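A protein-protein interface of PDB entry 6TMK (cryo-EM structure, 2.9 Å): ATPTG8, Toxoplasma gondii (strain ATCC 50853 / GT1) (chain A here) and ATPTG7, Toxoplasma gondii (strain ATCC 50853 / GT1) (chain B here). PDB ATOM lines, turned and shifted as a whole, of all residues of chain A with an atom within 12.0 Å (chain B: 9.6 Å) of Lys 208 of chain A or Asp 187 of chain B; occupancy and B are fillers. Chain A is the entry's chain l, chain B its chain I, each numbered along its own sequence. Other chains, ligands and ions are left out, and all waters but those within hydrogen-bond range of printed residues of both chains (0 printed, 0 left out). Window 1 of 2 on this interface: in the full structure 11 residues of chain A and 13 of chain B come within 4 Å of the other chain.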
ATOM      1  N   GLY A  27      -7.096 -14.977  13.054  1.00  0.00           N
ATOM      2  CA  GLY A  27      -6.198 -14.320  12.123  1.00  0.00           C
ATOM      3  C   GLY A  27      -6.642 -14.481  10.684  1.00  0.00           C
ATOM      4  O   GLY A  27      -6.523 -13.556   9.879  1.00  0.00           O
ATOM      5  N   GLU A  28      -7.157 -15.661  10.340  1.00  0.00           N
ATOM      6  CA  GLU A  28      -7.665 -15.883   8.992  1.00  0.00           C
ATOM      7  C   GLU A  28      -8.852 -14.973   8.699  1.00  0.00           C
ATOM      8  O   GLU A  28      -8.955 -14.400   7.606  1.00  0.00           O
ATOM      9  CB  GLU A  28      -8.054 -17.348   8.831  1.00  0.00           C
ATOM     10  CG  GLU A  28      -6.881 -18.301   8.969  1.00  0.00           C
ATOM     11  CD  GLU A  28      -7.310 -19.741   9.182  1.00  0.00           C
ATOM     12  OE1 GLU A  28      -8.500 -19.977   9.474  1.00  0.00           O
ATOM     13  OE2 GLU A  28      -6.452 -20.641   9.058  1.00  0.00           O
ATOM     14  N   ALA A  31      -7.533 -11.485   8.139  1.00  0.00           N
ATOM     15  CA  ALA A  31      -6.919 -11.395   6.820  1.00  0.00           C
ATOM     16  C   ALA A  31      -7.972 -11.296   5.726  1.00  0.00           C
ATOM     17  O   ALA A  31      -7.792 -10.569   4.742  1.00  0.00           O
ATOM     18  CB  ALA A  31      -6.013 -12.600   6.586  1.00  0.00           C
ATOM     19  N   ALA A  32      -9.075 -12.030   5.872  1.00  0.00           N
ATOM     20  CA  ALA A  32     -10.167 -11.922   4.910  1.00  0.00           C
ATOM     21  C   ALA A  32     -10.741 -10.511   4.883  1.00  0.00           C
ATOM     22  O   ALA A  32     -11.013  -9.953   3.808  1.00  0.00           O
ATOM     23  CB  ALA A  32     -11.256 -12.931   5.251  1.00  0.00           C
ATOM     24  N   LYS A  35      -8.442  -8.341   3.001  1.00  0.00           N
ATOM     25  CA  LYS A  35      -8.557  -8.569   1.566  1.00  0.00           C
ATOM     26  C   LYS A  35      -9.750  -7.821   0.985  1.00  0.00           C
ATOM     27  O   LYS A  35      -9.665  -7.245  -0.108  1.00  0.00           O
ATOM     28  CB  LYS A  35      -8.684 -10.065   1.296  1.00  0.00           C
ATOM     29  CG  LYS A  35      -7.478 -10.862   1.729  1.00  0.00           C
ATOM     30  CD  LYS A  35      -6.455 -10.988   0.631  1.00  0.00           C
ATOM     31  CE  LYS A  35      -5.247 -11.753   1.123  1.00  0.00           C
ATOM     32  NZ  LYS A  35      -5.562 -13.186   1.359  1.00  0.00           N
ATOM     33  N   LEU A  38      -8.898  -4.231   0.721  1.00  0.00           N
ATOM     34  CA  LEU A  38      -7.979  -4.017  -0.387  1.00  0.00           C
ATOM     35  C   LEU A  38      -8.716  -3.979  -1.714  1.00  0.00           C
ATOM     36  O   LEU A  38      -8.425  -3.137  -2.569  1.00  0.00           O
ATOM     37  CB  LEU A  38      -6.924  -5.113  -0.414  1.00  0.00           C
ATOM     38  CG  LEU A  38      -5.806  -5.046   0.613  1.00  0.00           C
ATOM     39  CD1 LEU A  38      -4.899  -6.226   0.407  1.00  0.00           C
ATOM     40  CD2 LEU A  38      -5.038  -3.760   0.485  1.00  0.00           C
ATOM     41  N   LEU A 201      -1.637  -1.725   4.055  1.00  0.00           N
ATOM     42  CA  LEU A 201      -2.399  -2.960   4.188  1.00  0.00           C
ATOM     43  C   LEU A 201      -1.704  -4.131   3.511  1.00  0.00           C
ATOM     44  O   LEU A 201      -1.875  -5.276   3.938  1.00  0.00           O
ATOM     45  CB  LEU A 201      -3.798  -2.793   3.609  1.00  0.00           C
ATOM     46  CG  LEU A 201      -4.797  -1.942   4.378  1.00  0.00           C
ATOM     47  CD1 LEU A 201      -6.155  -2.146   3.775  1.00  0.00           C
ATOM     48  CD2 LEU A 201      -4.810  -2.299   5.843  1.00  0.00           C
ATOM     49  N   LEU A 202      -0.922  -3.873   2.468  1.00  0.00           N
ATOM     50  CA  LEU A 202      -0.140  -4.937   1.857  1.00  0.00           C
ATOM     51  C   LEU A 202       1.082  -5.286   2.688  1.00  0.00           C
ATOM     52  O   LEU A 202       1.572  -6.418   2.619  1.00  0.00           O
ATOM     53  CB  LEU A 202       0.309  -4.529   0.459  1.00  0.00           C
ATOM     54  CG  LEU A 202      -0.748  -4.443  -0.635  1.00  0.00           C
ATOM     55  CD1 LEU A 202      -0.113  -3.934  -1.900  1.00  0.00           C
ATOM     56  CD2 LEU A 202      -1.406  -5.771  -0.868  1.00  0.00           C
ATOM     57  N   ASP A 203       1.587  -4.333   3.468  1.00  0.00           N
ATOM     58  CA  ASP A 203       2.618  -4.669   4.442  1.00  0.00           C
ATOM     59  C   ASP A 203       2.056  -5.511   5.579  1.00  0.00           C
ATOM     60  O   ASP A 203       2.770  -6.349   6.139  1.00  0.00           O
ATOM     61  CB  ASP A 203       3.250  -3.394   4.991  1.00  0.00           C
ATOM     62  CG  ASP A 203       4.375  -3.671   5.964  1.00  0.00           C
ATOM     63  OD1 ASP A 203       5.368  -4.309   5.560  1.00  0.00           O
ATOM     64  OD2 ASP A 203       4.266  -3.253   7.138  1.00  0.00           O
ATOM     65  N   LEU A 204       0.788  -5.308   5.929  1.00  0.00           N
ATOM     66  CA  LEU A 204       0.163  -6.079   6.996  1.00  0.00           C
ATOM     67  C   LEU A 204      -0.467  -7.381   6.525  1.00  0.00           C
ATOM     68  O   LEU A 204      -0.785  -8.235   7.359  1.00  0.00           O
ATOM     69  CB  LEU A 204      -0.918  -5.252   7.694  1.00  0.00           C
ATOM     70  CG  LEU A 204      -0.462  -4.024   8.473  1.00  0.00           C
ATOM     71  CD1 LEU A 204      -1.670  -3.307   9.036  1.00  0.00           C
ATOM     72  CD2 LEU A 204       0.486  -4.425   9.582  1.00  0.00           C
ATOM     73  N   VAL A 205      -0.669  -7.553   5.220  1.00  0.00           N
ATOM     74  CA  VAL A 205      -1.408  -8.714   4.743  1.00  0.00           C
ATOM     75  C   VAL A 205      -0.622  -9.990   5.020  1.00  0.00           C
ATOM     76  O   VAL A 205       0.607  -9.993   5.146  1.00  0.00           O
ATOM     77  CB  VAL A 205      -1.740  -8.578   3.249  1.00  0.00           C
ATOM     78  CG1 VAL A 205      -0.516  -8.836   2.405  1.00  0.00           C
ATOM     79  CG2 VAL A 205      -2.847  -9.523   2.869  1.00  0.00           C
ATOM     80  N   GLU A 206      -1.356 -11.094   5.110  1.00  0.00           N
ATOM     81  CA  GLU A 206      -0.838 -12.325   5.682  1.00  0.00           C
ATOM     82  C   GLU A 206      -1.434 -13.511   4.944  1.00  0.00           C
ATOM     83  O   GLU A 206      -2.635 -13.543   4.667  1.00  0.00           O
ATOM     84  CB  GLU A 206      -1.151 -12.425   7.177  1.00  0.00           C
ATOM     85  CG  GLU A 206      -0.417 -13.544   7.876  1.00  0.00           C
ATOM     86  CD  GLU A 206      -0.273 -13.306   9.364  1.00  0.00           C
ATOM     87  OE1 GLU A 206      -0.929 -12.382   9.886  1.00  0.00           O
ATOM     88  OE2 GLU A 206       0.500 -14.043  10.012  1.00  0.00           O
ATOM     89  N   GLY A 207      -0.583 -14.479   4.637  1.00  0.00           N
ATOM     90  CA  GLY A 207      -0.931 -15.628   3.834  1.00  0.00           C
ATOM     91  C   GLY A 207       0.119 -15.903   2.784  1.00  0.00           C
ATOM     92  O   GLY A 207       1.144 -15.229   2.692  1.00  0.00           O
ATOM     93  N   LYS A 208      -0.150 -16.922   1.979  1.00  0.00           N
ATOM     94  CA  LYS A 208       0.781 -17.326   0.937  1.00  0.00           C
ATOM     95  C   LYS A 208       0.073 -18.072  -0.183  1.00  0.00           C
ATOM     96  O   LYS A 208       0.428 -17.938  -1.353  1.00  0.00           O
ATOM     97  CB  LYS A 208       1.900 -18.178   1.539  1.00  0.00           C
ATOM     98  CG  LYS A 208       2.952 -18.634   0.544  1.00  0.00           C
ATOM     99  CD  LYS A 208       2.731 -20.064   0.097  1.00  0.00           C
ATOM    100  CE  LYS A 208       3.124 -21.039   1.192  1.00  0.00           C
ATOM    101  NZ  LYS A 208       2.841 -22.447   0.822  1.00  0.00           N
ATOM    102  OXT LYS A 208      -0.869 -18.825   0.058  1.00  0.00           O
ATOM    103  N   MET B 146       5.515 -14.607   7.696  1.00  0.00           N
ATOM    104  CA  MET B 146       4.650 -14.790   6.539  1.00  0.00           C
ATOM    105  C   MET B 146       4.177 -13.438   6.031  1.00  0.00           C
ATOM    106  O   MET B 146       3.957 -13.254   4.836  1.00  0.00           O
ATOM    107  CB  MET B 146       3.466 -15.684   6.895  1.00  0.00           C
ATOM    108  CG  MET B 146       2.660 -16.161   5.707  1.00  0.00           C
ATOM    109  SD  MET B 146       1.619 -17.578   6.108  1.00  0.00           S
ATOM    110  CE  MET B 146       0.361 -16.830   7.140  1.00  0.00           C
ATOM    111  N   SER B 147       4.014 -12.496   6.951  1.00  0.00           N
ATOM    112  CA  SER B 147       3.799 -11.104   6.597  1.00  0.00           C
ATOM    113  C   SER B 147       5.129 -10.360   6.556  1.00  0.00           C
ATOM    114  O   SER B 147       6.143 -10.809   7.097  1.00  0.00           O
ATOM    115  CB  SER B 147       2.850 -10.435   7.587  1.00  0.00           C
ATOM    116  OG  SER B 147       3.535  -9.992   8.740  1.00  0.00           O
ATOM    117  N   VAL B 148       5.112  -9.205   5.891  1.00  0.00           N
ATOM    118  CA  VAL B 148       6.331  -8.421   5.732  1.00  0.00           C
ATOM    119  C   VAL B 148       6.849  -7.957   7.086  1.00  0.00           C
ATOM    120  O   VAL B 148       8.058  -7.970   7.345  1.00  0.00           O
ATOM    121  CB  VAL B 148       6.074  -7.233   4.791  1.00  0.00           C
ATOM    122  CG1 VAL B 148       7.286  -6.348   4.717  1.00  0.00           C
ATOM    123  CG2 VAL B 148       5.693  -7.720   3.418  1.00  0.00           C
ATOM    124  N   GLU B 150       6.422  -9.452  10.033  1.00  0.00           N
ATOM    125  CA  GLU B 150       7.000 -10.599  10.722  1.00  0.00           C
ATOM    126  C   GLU B 150       8.359 -10.965  10.146  1.00  0.00           C
ATOM    127  O   GLU B 150       9.295 -11.270  10.893  1.00  0.00           O
ATOM    128  CB  GLU B 150       6.050 -11.786  10.626  1.00  0.00           C
ATOM    129  CG  GLU B 150       4.720 -11.566  11.312  1.00  0.00           C
ATOM    130  CD  GLU B 150       3.638 -12.490  10.792  1.00  0.00           C
ATOM    131  OE1 GLU B 150       2.444 -12.163  10.955  1.00  0.00           O
ATOM    132  OE2 GLU B 150       3.981 -13.544  10.217  1.00  0.00           O
ATOM    133  N   ALA B 151       8.494 -10.937   8.820  1.00  0.00           N
ATOM    134  CA  ALA B 151       9.770 -11.288   8.207  1.00  0.00           C
ATOM    135  C   ALA B 151      10.851 -10.274   8.551  1.00  0.00           C
ATOM    136  O   ALA B 151      12.006 -10.641   8.806  1.00  0.00           O
ATOM    137  CB  ALA B 151       9.603 -11.381   6.697  1.00  0.00           C
ATOM    138  N   SER B 154      11.950 -10.927  11.959  1.00  0.00           N
ATOM    139  CA  SER B 154      12.789 -12.117  11.945  1.00  0.00           C
ATOM    140  C   SER B 154      14.218 -11.771  11.553  1.00  0.00           C
ATOM    141  O   SER B 154      15.179 -12.230  12.181  1.00  0.00           O
ATOM    142  CB  SER B 154      12.205 -13.153  10.992  1.00  0.00           C
ATOM    143  OG  SER B 154      10.904 -13.535  11.399  1.00  0.00           O
ATOM    144  N   PHE B 155      14.378 -10.963  10.506  1.00  0.00           N
ATOM    145  CA  PHE B 155      15.722 -10.586  10.082  1.00  0.00           C
ATOM    146  C   PHE B 155      16.413  -9.707  11.115  1.00  0.00           C
ATOM    147  O   PHE B 155      17.638  -9.777  11.265  1.00  0.00           O
ATOM    148  CB  PHE B 155      15.670  -9.867   8.738  1.00  0.00           C
ATOM    149  CG  PHE B 155      15.574 -10.789   7.564  1.00  0.00           C
ATOM    150  CD1 PHE B 155      16.695 -11.437   7.087  1.00  0.00           C
ATOM    151  CD2 PHE B 155      14.365 -11.004   6.933  1.00  0.00           C
ATOM    152  CE1 PHE B 155      16.613 -12.284   6.007  1.00  0.00           C
ATOM    153  CE2 PHE B 155      14.278 -11.850   5.851  1.00  0.00           C
ATOM    154  CZ  PHE B 155      15.404 -12.490   5.387  1.00  0.00           C
ATOM    155  N   GLN B 179      16.565 -20.076   9.527  1.00  0.00           N
ATOM    156  CA  GLN B 179      15.540 -20.799   8.784  1.00  0.00           C
ATOM    157  C   GLN B 179      14.194 -20.094   8.875  1.00  0.00           C
ATOM    158  O   GLN B 179      13.466 -20.005   7.880  1.00  0.00           O
ATOM    159  CB  GLN B 179      15.429 -22.229   9.302  1.00  0.00           C
ATOM    160  CG  GLN B 179      16.658 -23.077   9.045  1.00  0.00           C
ATOM    161  CD  GLN B 179      16.985 -23.198   7.571  1.00  0.00           C
ATOM    162  OE1 GLN B 179      16.092 -23.213   6.725  1.00  0.00           O
ATOM    163  NE2 GLN B 179      18.271 -23.281   7.256  1.00  0.00           N
ATOM    164  N   ARG B 180      13.848 -19.581  10.055  1.00  0.00           N
ATOM    165  CA  ARG B 180      12.593 -18.853  10.204  1.00  0.00           C
ATOM    166  C   ARG B 180      12.568 -17.621   9.308  1.00  0.00           C
ATOM    167  O   ARG B 180      11.577 -17.359   8.612  1.00  0.00           O
ATOM    168  CB  ARG B 180      12.395 -18.464  11.666  1.00  0.00           C
ATOM    169  CG  ARG B 180      11.916 -19.606  12.546  1.00  0.00           C
ATOM    170  CD  ARG B 180      11.085 -19.111  13.717  1.00  0.00           C
ATOM    171  NE  ARG B 180      11.905 -18.444  14.728  1.00  0.00           N
ATOM    172  CZ  ARG B 180      12.125 -17.135  14.786  1.00  0.00           C
ATOM    173  NH1 ARG B 180      11.589 -16.315  13.893  1.00  0.00           N
ATOM    174  NH2 ARG B 180      12.888 -16.639  15.748  1.00  0.00           N
ATOM    175  N   ALA B 181      13.662 -16.859   9.304  1.00  0.00           N
ATOM    176  CA  ALA B 181      13.731 -15.660   8.481  1.00  0.00           C
ATOM    177  C   ALA B 181      13.608 -16.002   7.004  1.00  0.00           C
ATOM    178  O   ALA B 181      12.865 -15.349   6.260  1.00  0.00           O
ATOM    179  CB  ALA B 181      15.040 -14.924   8.752  1.00  0.00           C
ATOM    180  N   LEU B 182      14.338 -17.024   6.558  1.00  0.00           N
ATOM    181  CA  LEU B 182      14.285 -17.398   5.150  1.00  0.00           C
ATOM    182  C   LEU B 182      12.903 -17.901   4.761  1.00  0.00           C
ATOM    183  O   LEU B 182      12.418 -17.603   3.666  1.00  0.00           O
ATOM    184  CB  LEU B 182      15.339 -18.456   4.848  1.00  0.00           C
ATOM    185  CG  LEU B 182      16.796 -18.010   4.924  1.00  0.00           C
ATOM    186  CD1 LEU B 182      17.691 -19.176   4.608  1.00  0.00           C
ATOM    187  CD2 LEU B 182      17.075 -16.869   3.975  1.00  0.00           C
ATOM    188  N   GLN B 183      12.234 -18.630   5.654  1.00  0.00           N
ATOM    189  CA  GLN B 183      10.905 -19.135   5.332  1.00  0.00           C
ATOM    190  C   GLN B 183       9.894 -18.002   5.244  1.00  0.00           C
ATOM    191  O   GLN B 183       9.018 -18.008   4.370  1.00  0.00           O
ATOM    192  CB  GLN B 183      10.475 -20.159   6.380  1.00  0.00           C
ATOM    193  CG  GLN B 183       9.237 -20.950   6.017  1.00  0.00           C
ATOM    194  CD  GLN B 183       9.422 -21.788   4.771  1.00  0.00           C
ATOM    195  OE1 GLN B 183      10.022 -22.861   4.816  1.00  0.00           O
ATOM    196  NE2 GLN B 183       8.906 -21.303   3.649  1.00  0.00           N
ATOM    197  N   ALA B 184      10.005 -17.011   6.127  1.00  0.00           N
ATOM    198  CA  ALA B 184       9.095 -15.873   6.067  1.00  0.00           C
ATOM    199  C   ALA B 184       9.324 -15.054   4.802  1.00  0.00           C
ATOM    200  O   ALA B 184       8.369 -14.666   4.113  1.00  0.00           O
ATOM    201  CB  ALA B 184       9.267 -15.008   7.310  1.00  0.00           C
ATOM    202  N   ALA B 185      10.589 -14.776   4.482  1.00  0.00           N
ATOM    203  CA  ALA B 185      10.897 -14.075   3.241  1.00  0.00           C
ATOM    204  C   ALA B 185      10.401 -14.854   2.032  1.00  0.00           C
ATOM    205  O   ALA B 185       9.946 -14.265   1.047  1.00  0.00           O
ATOM    206  CB  ALA B 185      12.398 -13.830   3.144  1.00  0.00           C
ATOM    207  N   ALA B 186      10.470 -16.182   2.095  1.00  0.00           N
ATOM    208  CA  ALA B 186      10.004 -17.009   0.992  1.00  0.00           C
ATOM    209  C   ALA B 186       8.493 -16.939   0.843  1.00  0.00           C
ATOM    210  O   ALA B 186       7.973 -16.906  -0.277  1.00  0.00           O
ATOM    211  CB  ALA B 186      10.451 -18.445   1.213  1.00  0.00           C
ATOM    212  N   ASP B 187       7.772 -16.931   1.961  1.00  0.00           N
ATOM    213  CA  ASP B 187       6.328 -16.739   1.912  1.00  0.00           C
ATOM    214  C   ASP B 187       5.989 -15.404   1.261  1.00  0.00           C
ATOM    215  O   ASP B 187       5.104 -15.322   0.399  1.00  0.00           O
ATOM    216  CB  ASP B 187       5.746 -16.818   3.319  1.00  0.00           C
ATOM    217  CG  ASP B 187       6.035 -18.141   3.995  1.00  0.00           C
ATOM    218  OD1 ASP B 187       6.281 -18.144   5.219  1.00  0.00           O
ATOM    219  OD2 ASP B 187       6.021 -19.178   3.302  1.00  0.00           O
ATOM    220  N   VAL B 188       6.681 -14.343   1.675  1.00  0.00           N
ATOM    221  CA  VAL B 188       6.445 -13.030   1.084  1.00  0.00           C
ATOM    222  C   VAL B 188       6.709 -13.066  -0.416  1.00  0.00           C
ATOM    223  O   VAL B 188       5.933 -12.524  -1.213  1.00  0.00           O
ATOM    224  CB  VAL B 188       7.318 -11.973   1.779  1.00  0.00           C
ATOM    225  CG1 VAL B 188       7.259 -10.670   1.032  1.00  0.00           C
ATOM    226  CG2 VAL B 188       6.875 -11.788   3.197  1.00  0.00           C
ATOM    227  N   MET B 189       7.815 -13.689  -0.819  1.00  0.00           N
ATOM    228  CA  MET B 189       8.164 -13.749  -2.233  1.00  0.00           C
ATOM    229  C   MET B 189       7.105 -14.496  -3.022  1.00  0.00           C
ATOM    230  O   MET B 189       6.718 -14.070  -4.112  1.00  0.00           O
ATOM    231  CB  MET B 189       9.524 -14.414  -2.415  1.00  0.00           C
ATOM    232  CG  MET B 189      10.162 -14.165  -3.766  1.00  0.00           C
ATOM    233  SD  MET B 189       9.465 -15.163  -5.094  1.00  0.00           S
ATOM    234  CE  MET B 189       9.958 -16.805  -4.590  1.00  0.00           C
ATOM    235  N   SER B 190       6.647 -15.632  -2.502  1.00  0.00           N
ATOM    236  CA  SER B 190       5.647 -16.413  -3.216  1.00  0.00           C
ATOM    237  C   SER B 190       4.346 -15.639  -3.341  1.00  0.00           C
ATOM    238  O   SER B 190       3.690 -15.677  -4.388  1.00  0.00           O
ATOM    239  CB  SER B 190       5.417 -17.738  -2.499  1.00  0.00           C
ATOM    240  OG  SER B 190       6.463 -18.651  -2.770  1.00  0.00           O
ATOM    241  N   ARG B 191       3.948 -14.934  -2.283  1.00  0.00           N
ATOM    242  CA  ARG B 191       2.719 -14.154  -2.342  1.00  0.00           C
ATOM    243  C   ARG B 191       2.821 -13.020  -3.356  1.00  0.00           C
ATOM    244  O   ARG B 191       1.896 -12.794  -4.144  1.00  0.00           O
ATOM    245  CB  ARG B 191       2.395 -13.589  -0.963  1.00  0.00           C
ATOM    246  CG  ARG B 191       1.165 -12.724  -0.938  1.00  0.00           C
ATOM    247  CD  ARG B 191       0.699 -12.455   0.465  1.00  0.00           C
ATOM    248  NE  ARG B 191       1.620 -11.578   1.181  1.00  0.00           N
ATOM    249  CZ  ARG B 191       2.416 -11.954   2.176  1.00  0.00           C
ATOM    250  NH1 ARG B 191       2.436 -13.203   2.602  1.00  0.00           N
ATOM    251  NH2 ARG B 191       3.207 -11.065   2.747  1.00  0.00           N
ATOM    252  N   GLU B 192       3.937 -12.292  -3.352  1.00  0.00           N
ATOM    253  CA  GLU B 192       4.067 -11.106  -4.188  1.00  0.00           C
ATOM    254  C   GLU B 192       4.549 -11.387  -5.604  1.00  0.00           C
ATOM    255  O   GLU B 192       4.459 -10.497  -6.455  1.00  0.00           O
ATOM    256  CB  GLU B 192       5.021 -10.108  -3.531  1.00  0.00           C
ATOM    257  CG  GLU B 192       4.538  -9.575  -2.201  1.00  0.00           C
ATOM    258  CD  GLU B 192       5.379  -8.424  -1.692  1.00  0.00           C
ATOM    259  OE1 GLU B 192       5.065  -7.888  -0.609  1.00  0.00           O
ATOM    260  OE2 GLU B 192       6.355  -8.053  -2.376  1.00  0.00           O
ATOM    261  N   CYS B 193       5.053 -12.587  -5.886  1.00  0.00           N
ATOM    262  CA  CYS B 193       5.621 -12.906  -7.189  1.00  0.00           C
ATOM    263  C   CYS B 193       5.072 -14.215  -7.742  1.00  0.00           C
ATOM    264  O   CYS B 193       5.664 -14.789  -8.659  1.00  0.00           O
ATOM    265  CB  CYS B 193       7.147 -12.974  -7.102  1.00  0.00           C
ATOM    266  SG  CYS B 193       7.930 -11.585  -6.248  1.00  0.00           S
ATOM    267  N   GLY B 194       3.950 -14.695  -7.207  1.00  0.00           N
ATOM    268  CA  GLY B 194       3.383 -15.947  -7.672  1.00  0.00           C
ATOM    269  C   GLY B 194       2.716 -15.848  -9.027  1.00  0.00           C
ATOM    270  O   GLY B 194       2.745 -16.804  -9.806  1.00  0.00           O
ATOM    271  N   ALA B 195       2.098 -14.706  -9.325  1.00  0.00           N
ATOM    272  CA  ALA B 195       1.484 -14.516 -10.634  1.00  0.00           C
ATOM    273  C   ALA B 195       2.515 -14.612 -11.750  1.00  0.00           C
ATOM    274  O   ALA B 195       2.278 -15.265 -12.773  1.00  0.00           O
ATOM    275  CB  ALA B 195       0.775 -13.167 -10.684  1.00  0.00           C
ATOM    276  N   ASP B 198       3.647 -18.250 -12.148  1.00  0.00           N
ATOM    277  CA  ASP B 198       2.636 -19.022 -12.857  1.00  0.00           C
ATOM    278  C   ASP B 198       2.614 -18.671 -14.339  1.00  0.00           C
ATOM    279  O   ASP B 198       2.399 -19.543 -15.188  1.00  0.00           O
ATOM    280  CB  ASP B 198       1.268 -18.784 -12.224  1.00  0.00           C
ATOM    281  CG  ASP B 198       1.178 -19.322 -10.814  1.00  0.00           C
ATOM    282  OD1 ASP B 198       0.513 -18.681  -9.974  1.00  0.00           O
ATOM    283  OD2 ASP B 198       1.769 -20.386 -10.541  1.00  0.00           O
ATOM    284  N   VAL B 229      11.591  -7.613  -3.637  1.00  0.00           N
ATOM    285  CA  VAL B 229      11.258  -8.220  -2.353  1.00  0.00           C
ATOM    286  C   VAL B 229      12.496  -8.308  -1.470  1.00  0.00           C
ATOM    287  O   VAL B 229      12.458  -7.975  -0.279  1.00  0.00           O
ATOM    288  CB  VAL B 229      10.621  -9.603  -2.565  1.00  0.00           C
ATOM    289  CG1 VAL B 229      10.567 -10.358  -1.260  1.00  0.00           C
ATOM    290  CG2 VAL B 229       9.239  -9.452  -3.144  1.00  0.00           C
ATOM    291  N   LEU B 233      13.235  -6.480   2.128  1.00  0.00           N
ATOM    292  CA  LEU B 233      13.315  -7.276   3.346  1.00  0.00           C
ATOM    293  C   LEU B 233      14.670  -7.170   4.042  1.00  0.00           C
ATOM    294  O   LEU B 233      14.746  -6.725   5.191  1.00  0.00           O
ATOM    295  CB  LEU B 233      13.020  -8.743   3.029  1.00  0.00           C
ATOM    296  CG  LEU B 233      11.598  -9.062   2.585  1.00  0.00           C
ATOM    297  CD1 LEU B 233      11.509 -10.508   2.161  1.00  0.00           C
ATOM    298  CD2 LEU B 233      10.620  -8.772   3.692  1.00  0.00           C
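The guanidinium group of Arg 191 of chain B is in hydrogen-bond range of the backbone carbonyl oxygen of Gly 207 of chain A (2.4 Å). OE2 of Glu 206 of chain A lies close to OE1 of Glu 150 of chain B.
The backbone NH (N) of Met 146 of chain B lies within hydrogen-bond range of the side-chain carboxylate (OE2) of Glu 150 of chain B (3.1 Å). The backbone carbonyl oxygen (O) of Met 146 of chain B is in hydrogen-bond range of the guanidinium group (NH1) of Arg 191 of chain B (2.7 Å). The backbone NH (N) of Glu 150 of chain B lies within hydrogen-bond range of the side-chain hydroxyl (OG) of Ser 147 of chain B (3.2 Å). The side-chain hydroxyl of Ser 154 of chain B is in hydrogen-bond range of the backbone carbonyl oxygen of Glu 150 of chain B (2.8 Å).
Among the printed residues, pairs that only touch across the chains: Asp 203 of chain A with Val 148 of chain B, Val 205 of chain A with Ser 147 of chain B, Val 205 of chain A with Arg 191 of chain B, Glu 206 of chain A with Met 146 of chain B, Gly 207 of chain A with Met 146 of chain B and Lys 208 of chain A with Asp 187 of chain B.
Printed residues of chain B within 4 Å of Lys 208 of chain A: Asp 187. Asp 187 of chain B touches just one residue of chain A: Lys 208 (3.95 Å). Gly 207 of chain A touches just these residues of chain B: Met 146 (3.5 Å) and Arg 191 (2.4 Å). No residue of chain A comes within 4 Å of Ala 184 of chain B. No residue of chain A comes within 4 Å of Ala 186 of chain B. Val 188 of chain B touches none of the printed residues of chain A. Of the printed residues of chain B, Asp 203 of chain A touches Val 148 (2.9 Å). Printed residues of chain B within 4 Å of Val 205 of chain A: Ser 147 (3.3 Å) and Arg 191 (3.7 Å). Of the printed residues of chain B, Glu 206 of chain A touches Met 146 and Glu 150. Of the printed residues of chain A, Ser 147 of chain B touches Val 205. Leu 38 of chain A touches none of the printed residues of chain B. The nearest residue of chain A that does not touch Asp 187 of chain B is Gly 207 of chain A (4.6 Å). The nearest printed residue of chain A that does not touch Val 148 of chain B is Leu 202 of chain A (4.4 Å).
Of the 14 printed residues of chain A, 5 touch a printed residue of chain B. Printed residues of chain A that touch a printed residue of chain B: Asp 203, Val 205, Glu 206, Gly 207 and Lys 208. Among the printed residues, 8 pairs touch across the chains. Among the printed residues, no Asp or Glu carboxylate lies within 4 Å of a Lys or Arg side-chain nitrogen of the other chain.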
